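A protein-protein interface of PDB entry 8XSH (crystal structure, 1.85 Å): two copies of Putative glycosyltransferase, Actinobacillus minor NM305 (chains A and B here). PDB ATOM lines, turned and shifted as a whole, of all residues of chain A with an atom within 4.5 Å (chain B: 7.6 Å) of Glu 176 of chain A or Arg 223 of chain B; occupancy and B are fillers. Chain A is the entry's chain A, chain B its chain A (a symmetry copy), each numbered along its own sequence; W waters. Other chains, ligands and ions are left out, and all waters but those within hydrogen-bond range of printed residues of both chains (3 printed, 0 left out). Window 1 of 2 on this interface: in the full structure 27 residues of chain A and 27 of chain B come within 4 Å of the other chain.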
ATOM      1  N   ARG A 173     -11.415 -33.342   3.512  1.00  0.00           N
ATOM      2  CA  ARG A 173     -12.346 -32.455   2.824  1.00  0.00           C
ATOM      3  C   ARG A 173     -12.960 -33.181   1.632  1.00  0.00           C
ATOM      4  O   ARG A 173     -13.010 -32.636   0.522  1.00  0.00           O
ATOM      5  CB  ARG A 173     -11.636 -31.189   2.334  1.00  0.00           C
ATOM      6  CG  ARG A 173     -10.889 -30.392   3.382  1.00  0.00           C
ATOM      7  CD  ARG A 173     -10.555 -29.062   2.771  1.00  0.00           C
ATOM      8  NE  ARG A 173      -9.692 -28.260   3.613  1.00  0.00           N
ATOM      9  CZ  ARG A 173     -10.044 -27.177   4.281  1.00  0.00           C
ATOM     10  NH1 ARG A 173     -11.318 -26.858   4.389  1.00  0.00           N
ATOM     11  NH2 ARG A 173      -9.121 -26.464   4.911  1.00  0.00           N
ATOM     12  N   GLU A 174     -13.420 -34.416   1.839  1.00  0.00           N
ATOM     13  CA  GLU A 174     -13.916 -35.183   0.701  1.00  0.00           C
ATOM     14  C   GLU A 174     -14.991 -34.393  -0.049  1.00  0.00           C
ATOM     15  O   GLU A 174     -14.971 -34.273  -1.289  1.00  0.00           O
ATOM     16  CB  GLU A 174     -14.438 -36.553   1.133  1.00  0.00           C
ATOM     17  CG  GLU A 174     -15.304 -37.200   0.051  1.00  0.00           C
ATOM     18  CD  GLU A 174     -15.513 -38.695   0.182  1.00  0.00           C
ATOM     19  OE1 GLU A 174     -14.822 -39.328   1.027  1.00  0.00           O
ATOM     20  OE2 GLU A 174     -16.373 -39.214  -0.557  1.00  0.00           O
ATOM     21  N   GLU A 175     -15.947 -33.828   0.683  1.00  0.00           N
ATOM     22  CA  GLU A 175     -17.071 -33.183   0.008  1.00  0.00           C
ATOM     23  C   GLU A 175     -16.654 -31.851  -0.608  1.00  0.00           C
ATOM     24  O   GLU A 175     -17.205 -31.421  -1.625  1.00  0.00           O
ATOM     25  CB  GLU A 175     -18.212 -33.003   1.007  1.00  0.00           C
ATOM     26  CG  GLU A 175     -18.606 -34.325   1.590  1.00  0.00           C
ATOM     27  CD  GLU A 175     -20.070 -34.467   1.925  1.00  0.00           C
ATOM     28  OE1 GLU A 175     -20.877 -33.677   1.379  1.00  0.00           O
ATOM     29  OE2 GLU A 175     -20.398 -35.348   2.757  1.00  0.00           O
ATOM     30  N   GLU A 176     -15.627 -31.199  -0.059  1.00  0.00           N
ATOM     31  CA  GLU A 176     -15.248 -29.899  -0.593  1.00  0.00           C
ATOM     32  C   GLU A 176     -14.555 -30.025  -1.952  1.00  0.00           C
ATOM     33  O   GLU A 176     -14.642 -29.118  -2.799  1.00  0.00           O
ATOM     34  CB  GLU A 176     -14.367 -29.130   0.362  1.00  0.00           C
ATOM     35  CG  GLU A 176     -15.051 -28.827   1.692  1.00  0.00           C
ATOM     36  CD  GLU A 176     -14.196 -27.872   2.493  1.00  0.00           C
ATOM     37  OE1 GLU A 176     -13.959 -26.761   2.023  1.00  0.00           O
ATOM     38  OE2 GLU A 176     -13.699 -28.267   3.525  1.00  0.00           O
ATOM     39  N   SER A 177     -13.887 -31.140  -2.194  1.00  0.00           N
ATOM     40  CA  SER A 177     -13.300 -31.345  -3.510  1.00  0.00           C
ATOM     41  C   SER A 177     -14.368 -31.410  -4.610  1.00  0.00           C
ATOM     42  O   SER A 177     -14.147 -30.917  -5.729  1.00  0.00           O
ATOM     43  CB  SER A 177     -12.365 -32.555  -3.514  1.00  0.00           C
ATOM     44  OG  SER A 177     -13.083 -33.769  -3.505  1.00  0.00           O
ATOM     45  N   LYS A 178     -15.514 -32.025  -4.315  1.00  0.00           N
ATOM     46  CA  LYS A 178     -16.610 -32.062  -5.277  1.00  0.00           C
ATOM     47  C   LYS A 178     -17.134 -30.658  -5.552  1.00  0.00           C
ATOM     48  O   LYS A 178     -17.496 -30.328  -6.678  1.00  0.00           O
ATOM     49  CB  LYS A 178     -17.723 -32.977  -4.774  1.00  0.00           C
ATOM     50  CG  LYS A 178     -17.267 -34.412  -4.582  1.00  0.00           C
ATOM     51  CD  LYS A 178     -18.392 -35.341  -4.207  1.00  0.00           C
ATOM     52  CE  LYS A 178     -17.891 -36.728  -3.906  1.00  0.00           C
ATOM     53  NZ  LYS A 178     -19.031 -37.660  -3.749  1.00  0.00           N
ATOM     54  N   ILE A 179     -17.231 -29.838  -4.506  1.00  0.00           N
ATOM     55  CA  ILE A 179     -17.699 -28.468  -4.658  1.00  0.00           C
ATOM     56  C   ILE A 179     -16.731 -27.698  -5.546  1.00  0.00           C
ATOM     57  O   ILE A 179     -17.111 -27.009  -6.473  1.00  0.00           O
ATOM     58  CB  ILE A 179     -17.821 -27.802  -3.271  1.00  0.00           C
ATOM     59  CG1 ILE A 179     -18.862 -28.487  -2.368  1.00  0.00           C
ATOM     60  CG2 ILE A 179     -18.076 -26.316  -3.460  1.00  0.00           C
ATOM     61  CD1 ILE A 179     -18.865 -27.985  -0.917  1.00  0.00           C
ATOM     62  N   LEU A 180     -15.443 -27.775  -5.224  1.00  0.00           N
ATOM     63  CA  LEU A 180     -14.449 -27.058  -5.999  1.00  0.00           C
ATOM     64  C   LEU A 180     -14.499 -27.475  -7.470  1.00  0.00           C
ATOM     65  O   LEU A 180     -14.448 -26.611  -8.345  1.00  0.00           O
ATOM     66  CB  LEU A 180     -13.074 -27.310  -5.369  1.00  0.00           C
ATOM     67  CG  LEU A 180     -11.855 -26.687  -6.058  1.00  0.00           C
ATOM     68  CD1 LEU A 180     -11.437 -27.513  -7.272  1.00  0.00           C
ATOM     69  CD2 LEU A 180     -12.075 -25.228  -6.420  1.00  0.00           C
ATOM     70  N   PHE A 220      -6.250 -29.787  -0.621  1.00  0.00           N
ATOM     71  CA  PHE A 220      -7.415 -29.898   0.247  1.00  0.00           C
ATOM     72  C   PHE A 220      -6.953 -30.158   1.686  1.00  0.00           C
ATOM     73  O   PHE A 220      -7.656 -30.784   2.479  1.00  0.00           O
ATOM     74  CB  PHE A 220      -8.379 -30.951  -0.290  1.00  0.00           C
ATOM     75  CG  PHE A 220      -9.095 -30.487  -1.541  1.00  0.00           C
ATOM     76  CD1 PHE A 220     -10.072 -29.520  -1.487  1.00  0.00           C
ATOM     77  CD2 PHE A 220      -8.634 -30.875  -2.801  1.00  0.00           C
ATOM     78  CE1 PHE A 220     -10.673 -29.039  -2.642  1.00  0.00           C
ATOM     79  CE2 PHE A 220      -9.209 -30.370  -3.961  1.00  0.00           C
ATOM     80  CZ  PHE A 220     -10.224 -29.446  -3.888  1.00  0.00           C
ATOM     81  N   PHE A 243      -6.220 -24.870  -0.474  1.00  0.00           N
ATOM     82  CA  PHE A 243      -6.201 -24.665   0.962  1.00  0.00           C
ATOM     83  C   PHE A 243      -4.813 -24.927   1.528  1.00  0.00           C
ATOM     84  O   PHE A 243      -4.143 -25.896   1.156  1.00  0.00           O
ATOM     85  CB  PHE A 243      -7.240 -25.554   1.647  1.00  0.00           C
ATOM     86  CG  PHE A 243      -8.660 -25.297   1.201  1.00  0.00           C
ATOM     87  CD1 PHE A 243      -9.230 -24.055   1.369  1.00  0.00           C
ATOM     88  CD2 PHE A 243      -9.396 -26.264   0.557  1.00  0.00           C
ATOM     89  CE1 PHE A 243     -10.548 -23.817   0.985  1.00  0.00           C
ATOM     90  CE2 PHE A 243     -10.719 -26.031   0.179  1.00  0.00           C
ATOM     91  CZ  PHE A 243     -11.286 -24.805   0.381  1.00  0.00           C
ATOM     92  N   TYR A 268     -14.152 -21.063  -2.723  1.00  0.00           N
ATOM     93  CA  TYR A 268     -14.151 -22.006  -3.840  1.00  0.00           C
ATOM     94  C   TYR A 268     -13.996 -21.299  -5.184  1.00  0.00           C
ATOM     95  O   TYR A 268     -13.331 -21.797  -6.087  1.00  0.00           O
ATOM     96  CB  TYR A 268     -15.443 -22.827  -3.862  1.00  0.00           C
ATOM     97  CG  TYR A 268     -15.640 -23.615  -2.595  1.00  0.00           C
ATOM     98  CD1 TYR A 268     -14.796 -24.666  -2.259  1.00  0.00           C
ATOM     99  CD2 TYR A 268     -16.645 -23.280  -1.702  1.00  0.00           C
ATOM    100  CE1 TYR A 268     -14.941 -25.350  -1.050  1.00  0.00           C
ATOM    101  CE2 TYR A 268     -16.803 -23.960  -0.506  1.00  0.00           C
ATOM    102  CZ  TYR A 268     -15.992 -25.029  -0.210  1.00  0.00           C
ATOM    103  OH  TYR A 268     -16.163 -25.659   0.986  1.00  0.00           O
ATOM    104  N   GLN B 100     -32.277 -26.529  -2.201  1.00  0.00           N
ATOM    105  CA  GLN B 100     -32.204 -26.321  -0.768  1.00  0.00           C
ATOM    106  C   GLN B 100     -30.790 -26.498  -0.215  1.00  0.00           C
ATOM    107  O   GLN B 100     -30.584 -26.339   0.993  1.00  0.00           O
ATOM    108  CB  GLN B 100     -33.125 -27.309  -0.051  1.00  0.00           C
ATOM    109  CG  GLN B 100     -34.575 -27.174  -0.477  1.00  0.00           C
ATOM    110  CD  GLN B 100     -35.504 -27.977   0.384  1.00  0.00           C
ATOM    111  OE1 GLN B 100     -36.175 -28.896  -0.074  1.00  0.00           O
ATOM    112  NE2 GLN B 100     -35.572 -27.600   1.642  1.00  0.00           N
ATOM    113  N   ASN B 101     -29.838 -26.832  -1.077  1.00  0.00           N
ATOM    114  CA  ASN B 101     -28.509 -27.234  -0.673  1.00  0.00           C
ATOM    115  C   ASN B 101     -27.536 -26.790  -1.754  1.00  0.00           C
ATOM    116  O   ASN B 101     -27.101 -27.604  -2.549  1.00  0.00           O
ATOM    117  CB  ASN B 101     -28.396 -28.747  -0.451  1.00  0.00           C
ATOM    118  CG  ASN B 101     -29.319 -29.283   0.635  1.00  0.00           C
ATOM    119  OD1 ASN B 101     -29.080 -29.078   1.824  1.00  0.00           O
ATOM    120  ND2 ASN B 101     -30.396 -29.958   0.234  1.00  0.00           N
ATOM    121  N   PRO B 102     -27.169 -25.502  -1.835  1.00  0.00           N
ATOM    122  CA  PRO B 102     -26.377 -25.016  -2.971  1.00  0.00           C
ATOM    123  C   PRO B 102     -25.031 -25.711  -3.160  1.00  0.00           C
ATOM    124  O   PRO B 102     -24.510 -25.818  -4.271  1.00  0.00           O
ATOM    125  CB  PRO B 102     -26.161 -23.534  -2.655  1.00  0.00           C
ATOM    126  CG  PRO B 102     -26.438 -23.413  -1.163  1.00  0.00           C
ATOM    127  CD  PRO B 102     -27.481 -24.448  -0.862  1.00  0.00           C
ATOM    128  N   PHE B 103     -24.434 -26.150  -2.048  1.00  0.00           N
ATOM    129  CA  PHE B 103     -23.149 -26.816  -2.120  1.00  0.00           C
ATOM    130  C   PHE B 103     -23.325 -28.246  -2.623  1.00  0.00           C
ATOM    131  O   PHE B 103     -22.336 -28.872  -2.949  1.00  0.00           O
ATOM    132  CB  PHE B 103     -22.435 -26.756  -0.772  1.00  0.00           C
ATOM    133  CG  PHE B 103     -22.095 -25.358  -0.340  1.00  0.00           C
ATOM    134  CD1 PHE B 103     -21.045 -24.667  -0.933  1.00  0.00           C
ATOM    135  CD2 PHE B 103     -22.831 -24.715   0.644  1.00  0.00           C
ATOM    136  CE1 PHE B 103     -20.711 -23.389  -0.528  1.00  0.00           C
ATOM    137  CE2 PHE B 103     -22.497 -23.429   1.043  1.00  0.00           C
ATOM    138  CZ  PHE B 103     -21.424 -22.775   0.476  1.00  0.00           C
ATOM    139  N   TYR B 104     -24.555 -28.739  -2.779  1.00  0.00           N
ATOM    140  CA  TYR B 104     -24.743 -30.056  -3.345  1.00  0.00           C
ATOM    141  C   TYR B 104     -25.299 -29.963  -4.752  1.00  0.00           C
ATOM    142  O   TYR B 104     -25.804 -30.962  -5.271  1.00  0.00           O
ATOM    143  CB  TYR B 104     -25.653 -30.904  -2.463  1.00  0.00           C
ATOM    144  CG  TYR B 104     -24.963 -31.395  -1.222  1.00  0.00           C
ATOM    145  CD1 TYR B 104     -24.165 -32.538  -1.223  1.00  0.00           C
ATOM    146  CD2 TYR B 104     -25.027 -30.665  -0.059  1.00  0.00           C
ATOM    147  CE1 TYR B 104     -23.513 -32.962  -0.070  1.00  0.00           C
ATOM    148  CE2 TYR B 104     -24.397 -31.078   1.102  1.00  0.00           C
ATOM    149  CZ  TYR B 104     -23.633 -32.227   1.100  1.00  0.00           C
ATOM    150  OH  TYR B 104     -22.984 -32.599   2.270  1.00  0.00           O
ATOM    151  N   HIS B 106     -23.774 -29.987  -7.325  1.00  0.00           N
ATOM    152  CA  HIS B 106     -22.991 -30.912  -8.141  1.00  0.00           C
ATOM    153  C   HIS B 106     -23.580 -32.320  -8.191  1.00  0.00           C
ATOM    154  O   HIS B 106     -23.173 -33.128  -9.036  1.00  0.00           O
ATOM    155  CB  HIS B 106     -21.533 -30.941  -7.669  1.00  0.00           C
ATOM    156  CG  HIS B 106     -21.381 -31.496  -6.320  1.00  0.00           C
ATOM    157  ND1 HIS B 106     -21.528 -32.837  -6.027  1.00  0.00           N
ATOM    158  CD2 HIS B 106     -21.182 -30.860  -5.156  1.00  0.00           C
ATOM    159  CE1 HIS B 106     -21.381 -32.995  -4.722  1.00  0.00           C
ATOM    160  NE2 HIS B 106     -21.177 -31.810  -4.179  1.00  0.00           N
ATOM    161  N   TYR B 129     -28.852 -15.512   0.845  1.00  0.00           N
ATOM    162  CA  TYR B 129     -27.496 -16.045   0.764  1.00  0.00           C
ATOM    163  C   TYR B 129     -27.360 -17.108  -0.344  1.00  0.00           C
ATOM    164  O   TYR B 129     -26.423 -17.063  -1.133  1.00  0.00           O
ATOM    165  CB  TYR B 129     -27.065 -16.664   2.085  1.00  0.00           C
ATOM    166  CG  TYR B 129     -25.719 -17.350   2.038  1.00  0.00           C
ATOM    167  CD1 TYR B 129     -24.552 -16.648   2.279  1.00  0.00           C
ATOM    168  CD2 TYR B 129     -25.619 -18.691   1.745  1.00  0.00           C
ATOM    169  CE1 TYR B 129     -23.317 -17.280   2.271  1.00  0.00           C
ATOM    170  CE2 TYR B 129     -24.392 -19.335   1.702  1.00  0.00           C
ATOM    171  CZ  TYR B 129     -23.232 -18.627   1.992  1.00  0.00           C
ATOM    172  OH  TYR B 129     -21.987 -19.222   1.947  1.00  0.00           O
ATOM    173  N   LYS B 172     -22.595 -32.261  11.580  1.00  0.00           N
ATOM    174  CA  LYS B 172     -21.498 -31.671  10.848  1.00  0.00           C
ATOM    175  C   LYS B 172     -20.347 -31.425  11.825  1.00  0.00           C
ATOM    176  O   LYS B 172     -20.542 -31.201  13.039  1.00  0.00           O
ATOM    177  CB  LYS B 172     -21.971 -30.392  10.156  1.00  0.00           C
ATOM    178  CG  LYS B 172     -23.270 -30.559   9.377  1.00  0.00           C
ATOM    179  CD  LYS B 172     -23.622 -29.371   8.565  1.00  0.00           C
ATOM    180  CE  LYS B 172     -24.821 -29.596   7.683  1.00  0.00           C
ATOM    181  NZ  LYS B 172     -24.874 -28.516   6.681  1.00  0.00           N
ATOM    182  N   ARG B 173     -19.151 -31.506  11.266  1.00  0.00           N
ATOM    183  CA  ARG B 173     -17.916 -31.180  11.970  1.00  0.00           C
ATOM    184  C   ARG B 173     -17.724 -32.138  13.140  1.00  0.00           C
ATOM    185  O   ARG B 173     -17.430 -31.709  14.263  1.00  0.00           O
ATOM    186  CB  ARG B 173     -17.948 -29.740  12.495  1.00  0.00           C
ATOM    187  CG  ARG B 173     -18.225 -28.661  11.472  1.00  0.00           C
ATOM    188  CD  ARG B 173     -17.897 -27.345  12.118  1.00  0.00           C
ATOM    189  NE  ARG B 173     -18.275 -26.211  11.301  1.00  0.00           N
ATOM    190  CZ  ARG B 173     -17.450 -25.405  10.657  1.00  0.00           C
ATOM    191  NH1 ARG B 173     -16.175 -25.722  10.549  1.00  0.00           N
ATOM    192  NH2 ARG B 173     -17.924 -24.327  10.051  1.00  0.00           N
ATOM    193  N   PHE B 220     -22.056 -26.040  15.517  1.00  0.00           N
ATOM    194  CA  PHE B 220     -21.075 -26.665  14.640  1.00  0.00           C
ATOM    195  C   PHE B 220     -21.597 -26.641  13.197  1.00  0.00           C
ATOM    196  O   PHE B 220     -21.267 -27.505  12.385  1.00  0.00           O
ATOM    197  CB  PHE B 220     -20.725 -28.061  15.144  1.00  0.00           C
ATOM    198  CG  PHE B 220     -19.882 -28.020  16.402  1.00  0.00           C
ATOM    199  CD1 PHE B 220     -18.565 -27.626  16.365  1.00  0.00           C
ATOM    200  CD2 PHE B 220     -20.480 -28.176  17.654  1.00  0.00           C
ATOM    201  CE1 PHE B 220     -17.816 -27.514  17.529  1.00  0.00           C
ATOM    202  CE2 PHE B 220     -19.742 -28.030  18.823  1.00  0.00           C
ATOM    203  CZ  PHE B 220     -18.411 -27.692  18.767  1.00  0.00           C
ATOM    204  N   ALA B 221     -22.411 -25.626  12.899  1.00  0.00           N
ATOM    205  CA  ALA B 221     -22.964 -25.405  11.573  1.00  0.00           C
ATOM    206  C   ALA B 221     -21.854 -25.304  10.529  1.00  0.00           C
ATOM    207  O   ALA B 221     -20.756 -24.800  10.818  1.00  0.00           O
ATOM    208  CB  ALA B 221     -23.712 -24.131  11.606  1.00  0.00           C
ATOM    209  N   GLU B 222     -22.174 -25.720   9.306  1.00  0.00           N
ATOM    210  CA  GLU B 222     -21.166 -25.823   8.266  1.00  0.00           C
ATOM    211  C   GLU B 222     -21.845 -25.770   6.898  1.00  0.00           C
ATOM    212  O   GLU B 222     -22.718 -26.578   6.622  1.00  0.00           O
ATOM    213  CB  GLU B 222     -20.415 -27.143   8.391  1.00  0.00           C
ATOM    214  CG  GLU B 222     -19.268 -27.312   7.414  1.00  0.00           C
ATOM    215  CD  GLU B 222     -18.588 -28.663   7.545  1.00  0.00           C
ATOM    216  OE1 GLU B 222     -19.297 -29.690   7.480  1.00  0.00           O
ATOM    217  OE2 GLU B 222     -17.382 -28.695   7.734  1.00  0.00           O
ATOM    218  N   ARG B 223     -21.429 -24.800   6.079  1.00  0.00           N
ATOM    219  CA  ARG B 223     -21.951 -24.599   4.736  1.00  0.00           C
ATOM    220  C   ARG B 223     -23.477 -24.616   4.715  1.00  0.00           C
ATOM    221  O   ARG B 223     -24.115 -25.343   3.942  1.00  0.00           O
ATOM    222  CB  ARG B 223     -21.319 -25.604   3.779  1.00  0.00           C
ATOM    223  CG  ARG B 223     -19.880 -25.225   3.439  1.00  0.00           C
ATOM    224  CD  ARG B 223     -19.256 -26.099   2.351  1.00  0.00           C
ATOM    225  NE  ARG B 223     -18.995 -27.468   2.786  1.00  0.00           N
ATOM    226  CZ  ARG B 223     -18.019 -27.847   3.600  1.00  0.00           C
ATOM    227  NH1 ARG B 223     -17.089 -26.996   3.990  1.00  0.00           N
ATOM    228  NH2 ARG B 223     -17.957 -29.092   4.020  1.00  0.00           N
ATOM    229  N   GLU B 224     -24.035 -23.707   5.516  1.00  0.00           N
ATOM    230  CA  GLU B 224     -25.474 -23.601   5.661  1.00  0.00           C
ATOM    231  C   GLU B 224     -26.041 -22.752   4.528  1.00  0.00           C
ATOM    232  O   GLU B 224     -25.340 -21.938   3.929  1.00  0.00           O
ATOM    233  CB  GLU B 224     -25.802 -23.005   7.032  1.00  0.00           C
ATOM    234  CG  GLU B 224     -25.250 -23.833   8.205  1.00  0.00           C
ATOM    235  CD  GLU B 224     -25.749 -25.271   8.322  1.00  0.00           C
ATOM    236  OE1 GLU B 224     -26.776 -25.565   7.707  1.00  0.00           O
ATOM    237  OE2 GLU B 224     -25.061 -26.158   8.908  1.00  0.00           O
ATOM    238  N   SER B 225     -27.335 -22.934   4.272  1.00  0.00           N
ATOM    239  CA  SER B 225     -28.075 -22.029   3.407  1.00  0.00           C
ATOM    240  C   SER B 225     -28.757 -20.947   4.256  1.00  0.00           C
ATOM    241  O   SER B 225     -28.723 -19.754   3.932  1.00  0.00           O
ATOM    242  CB  SER B 225     -29.071 -22.806   2.584  1.00  0.00           C
ATOM    243  OG  SER B 225     -29.931 -23.589   3.410  1.00  0.00           O
ATOM    244  N   LEU B 226     -29.327 -21.389   5.377  1.00  0.00           N
ATOM    245  CA  LEU B 226     -30.065 -20.501   6.261  1.00  0.00           C
ATOM    246  C   LEU B 226     -29.559 -20.634   7.685  1.00  0.00           C
ATOM    247  O   LEU B 226     -29.353 -19.610   8.346  1.00  0.00           O
ATOM    248  CB  LEU B 226     -31.564 -20.807   6.148  1.00  0.00           C
ATOM    249  CG  LEU B 226     -32.481 -19.941   7.000  1.00  0.00           C
ATOM    250  CD1 LEU B 226     -32.340 -18.460   6.684  1.00  0.00           C
ATOM    251  CD2 LEU B 226     -33.932 -20.377   6.863  1.00  0.00           C
ATOM    252  N   GLY B 227     -29.388 -21.869   8.155  1.00  0.00           N
ATOM    253  CA  GLY B 227     -28.909 -22.112   9.507  1.00  0.00           C
ATOM    254  C   GLY B 227     -30.035 -22.550  10.432  1.00  0.00           C
ATOM    255  O   GLY B 227     -30.211 -21.975  11.502  1.00  0.00           O
ATOM    256  N   SER B 244     -20.982 -20.031  12.607  1.00  0.00           N
ATOM    257  CA  SER B 244     -22.185 -19.507  11.976  1.00  0.00           C
ATOM    258  C   SER B 244     -22.701 -20.439  10.880  1.00  0.00           C
ATOM    259  O   SER B 244     -23.890 -20.444  10.613  1.00  0.00           O
ATOM    260  CB  SER B 244     -21.953 -18.152  11.362  1.00  0.00           C
ATOM    261  OG  SER B 244     -20.997 -18.226  10.295  1.00  0.00           O
ATOM    262  N   GLY B 245     -21.815 -21.181  10.224  1.00  0.00           N
ATOM    263  CA  GLY B 245     -22.225 -21.944   9.054  1.00  0.00           C
ATOM    264  C   GLY B 245     -21.943 -21.195   7.747  1.00  0.00           C
ATOM    265  O   GLY B 245     -22.271 -21.714   6.698  1.00  0.00           O
ATOM    266  N   PHE B 246     -21.388 -19.987   7.829  1.00  0.00           N
ATOM    267  CA  PHE B 246     -21.149 -19.126   6.677  1.00  0.00           C
ATOM    268  C   PHE B 246     -19.729 -18.573   6.749  1.00  0.00           C
ATOM    269  O   PHE B 246     -19.444 -17.645   7.526  1.00  0.00           O
ATOM    270  CB  PHE B 246     -22.157 -17.962   6.640  1.00  0.00           C
ATOM    271  CG  PHE B 246     -23.601 -18.387   6.661  1.00  0.00           C
ATOM    272  CD1 PHE B 246     -24.255 -18.633   7.858  1.00  0.00           C
ATOM    273  CD2 PHE B 246     -24.292 -18.615   5.486  1.00  0.00           C
ATOM    274  CE1 PHE B 246     -25.586 -19.024   7.858  1.00  0.00           C
ATOM    275  CE2 PHE B 246     -25.612 -19.041   5.488  1.00  0.00           C
ATOM    276  CZ  PHE B 246     -26.268 -19.221   6.682  1.00  0.00           C
ATOM    277  N   THR B 247     -18.838 -19.134   5.924  1.00  0.00           N
ATOM    278  CA  THR B 247     -17.500 -18.599   5.844  1.00  0.00           C
ATOM    279  C   THR B 247     -17.559 -17.168   5.344  1.00  0.00           C
ATOM    280  O   THR B 247     -16.832 -16.312   5.833  1.00  0.00           O
ATOM    281  CB  THR B 247     -16.597 -19.462   4.954  1.00  0.00           C
ATOM    282  OG1 THR B 247     -17.141 -19.543   3.631  1.00  0.00           O
ATOM    283  CG2 THR B 247     -16.364 -20.849   5.519  1.00  0.00           C
ATOM    284  N   ASP B 248     -18.392 -16.931   4.341  1.00  0.00           N
ATOM    285  CA  ASP B 248     -18.629 -15.623   3.760  1.00  0.00           C
ATOM    286  C   ASP B 248     -19.827 -15.003   4.485  1.00  0.00           C
ATOM    287  O   ASP B 248     -20.884 -14.755   3.889  1.00  0.00           O
ATOM    288  CB  ASP B 248     -18.766 -15.764   2.242  1.00  0.00           C
ATOM    289  CG  ASP B 248     -19.853 -16.725   1.749  1.00  0.00           C
ATOM    290  OD1 ASP B 248     -20.107 -17.763   2.428  1.00  0.00           O
ATOM    291  OD2 ASP B 248     -20.413 -16.469   0.666  1.00  0.00           O
ATOM    292  N   GLU B 265     -13.689 -19.872  11.244  1.00  0.00           N
ATOM    293  CA  GLU B 265     -13.093 -21.191  11.138  1.00  0.00           C
ATOM    294  C   GLU B 265     -11.815 -21.241  11.954  1.00  0.00           C
ATOM    295  O   GLU B 265     -11.038 -20.295  11.910  1.00  0.00           O
ATOM    296  CB  GLU B 265     -12.707 -21.523   9.709  1.00  0.00           C
ATOM    297  CG  GLU B 265     -13.889 -21.599   8.796  1.00  0.00           C
ATOM    298  CD  GLU B 265     -14.758 -22.820   8.980  1.00  0.00           C
ATOM    299  OE1 GLU B 265     -14.220 -23.881   9.356  1.00  0.00           O
ATOM    300  OE2 GLU B 265     -15.955 -22.708   8.706  1.00  0.00           O
HETATM  301  O   HOH W   1     -20.142 -31.911  -1.409  1.00  0.00           O
HETATM  302  O   HOH W   2     -16.615 -24.038   3.667  1.00  0.00           O
HETATM  303  O   HOH W   3     -20.131 -31.220   3.573  1.00  0.00           O
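The side-chain carboxylate of Glu 175 of chain A is in hydrogen-bond range of the side-chain hydroxyl of Tyr 104 of chain B (2.5 Å). The guanidinium group (NH1) of Arg 223 of chain B is in salt-bridge range of the side-chain carboxylate (OE2) of Glu 176 of chain A, at 3.7 Å. The side-chain hydroxyl of Tyr 268 of chain A sits close to the guanidinium group of Arg 223 of chain B, 3.4 Å away.
The guanidinium group of Arg 173 of chain A is in salt-bridge range of the side-chain carboxylate of Glu 176 of chain A (2.9 Å). OE1 of Glu 176 of chain A lies within hydrogen-bond range of OH of Tyr 268 of chain A, 2.7 Å away. The backbone carbonyl oxygen (O) of Phe 103 of chain B lies close to a ring nitrogen (NE2) of His 106 of chain B, at 3.4 Å. OE1 of Glu 222 of chain B is in salt-bridge range of NH2 of Arg 223 of chain B. N of Arg 223 of chain B is in hydrogen-bond range of O of Gly 245 of chain B (3.3 Å).
CE1 of His 106 of chain B touches CB of Lys 178 of chain A (3.7 Å). CG1 of Ile 179 of chain A touches O of Phe 103 of chain B (3.5 Å). CD1 of Ile 179 of chain A touches NE of Arg 223 of chain B, 3.7 Å away. Tyr 268 of chain A touches Phe 103 of chain B (CE2 to CE1, 3.9 Å).
Of chain B, only Arg 223 comes within 4 Å of Glu 176 of chain A. Of chain A, only Glu 176, Ile 179 and Tyr 268 come within 4 Å of Arg 223 of chain B. Printed residues of chain A within 4 Å of His 106 of chain B: Lys 178. Printed residues of chain B within 4 Å of Ile 179 of chain A: Phe 103 and Arg 223. Printed residues of chain B within 4 Å of Glu 175 of chain A: Tyr 104. Printed residues of chain B within 4 Å of Tyr 268 of chain A: Phe 103 (3.9 Å) and Arg 223 (3.4 Å). Printed residues of chain A within 4 Å of Phe 103 of chain B: Ile 179 (3.5 Å) and Tyr 268 (3.9 Å). Thr 247 of chain B touches none of the printed residues of chain A. Ser 244 of chain B touches none of the printed residues of chain A. The nearest printed residue of chain A that does not touch Arg 223 of chain B is Glu 175 of chain A (4.9 Å). The nearest printed residue of chain A that does not touch Tyr 104 of chain B is Ile 179 of chain A (5.7 Å).
Hydrophobic or aromatic side chains of chain A that line the printed part of chain B: Ile 179 and Tyr 268. Printed residues of chain B that touch a printed residue of chain A: Phe 103, Tyr 104, His 106 and Arg 223. Among the printed residues, 7 pairs touch across the chains. Among the printed residues, Asp or Glu carboxylates within 4 Å of a Lys or Arg side-chain nitrogen of the other chain: Glu 176 of chain A with Arg 223 of chain B (3.7 Å).
Positions printed for both chains: 173 and 220.
Water W1 bridges a ring nitrogen (NE2) of His 106 of chain B and the backbone carbonyl oxygen of Glu 175 of chain A. Water W2 bridges the guanidinium group (NH1) of Arg 223 of chain B and the side-chain hydroxyl (OH) of Tyr 268 of chain A. Water W3 lies within hydrogen-bond range of NH2 of Arg 223 of chain B, OE1 of Glu 175 of chain A and OH of Tyr 104 of chain B.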
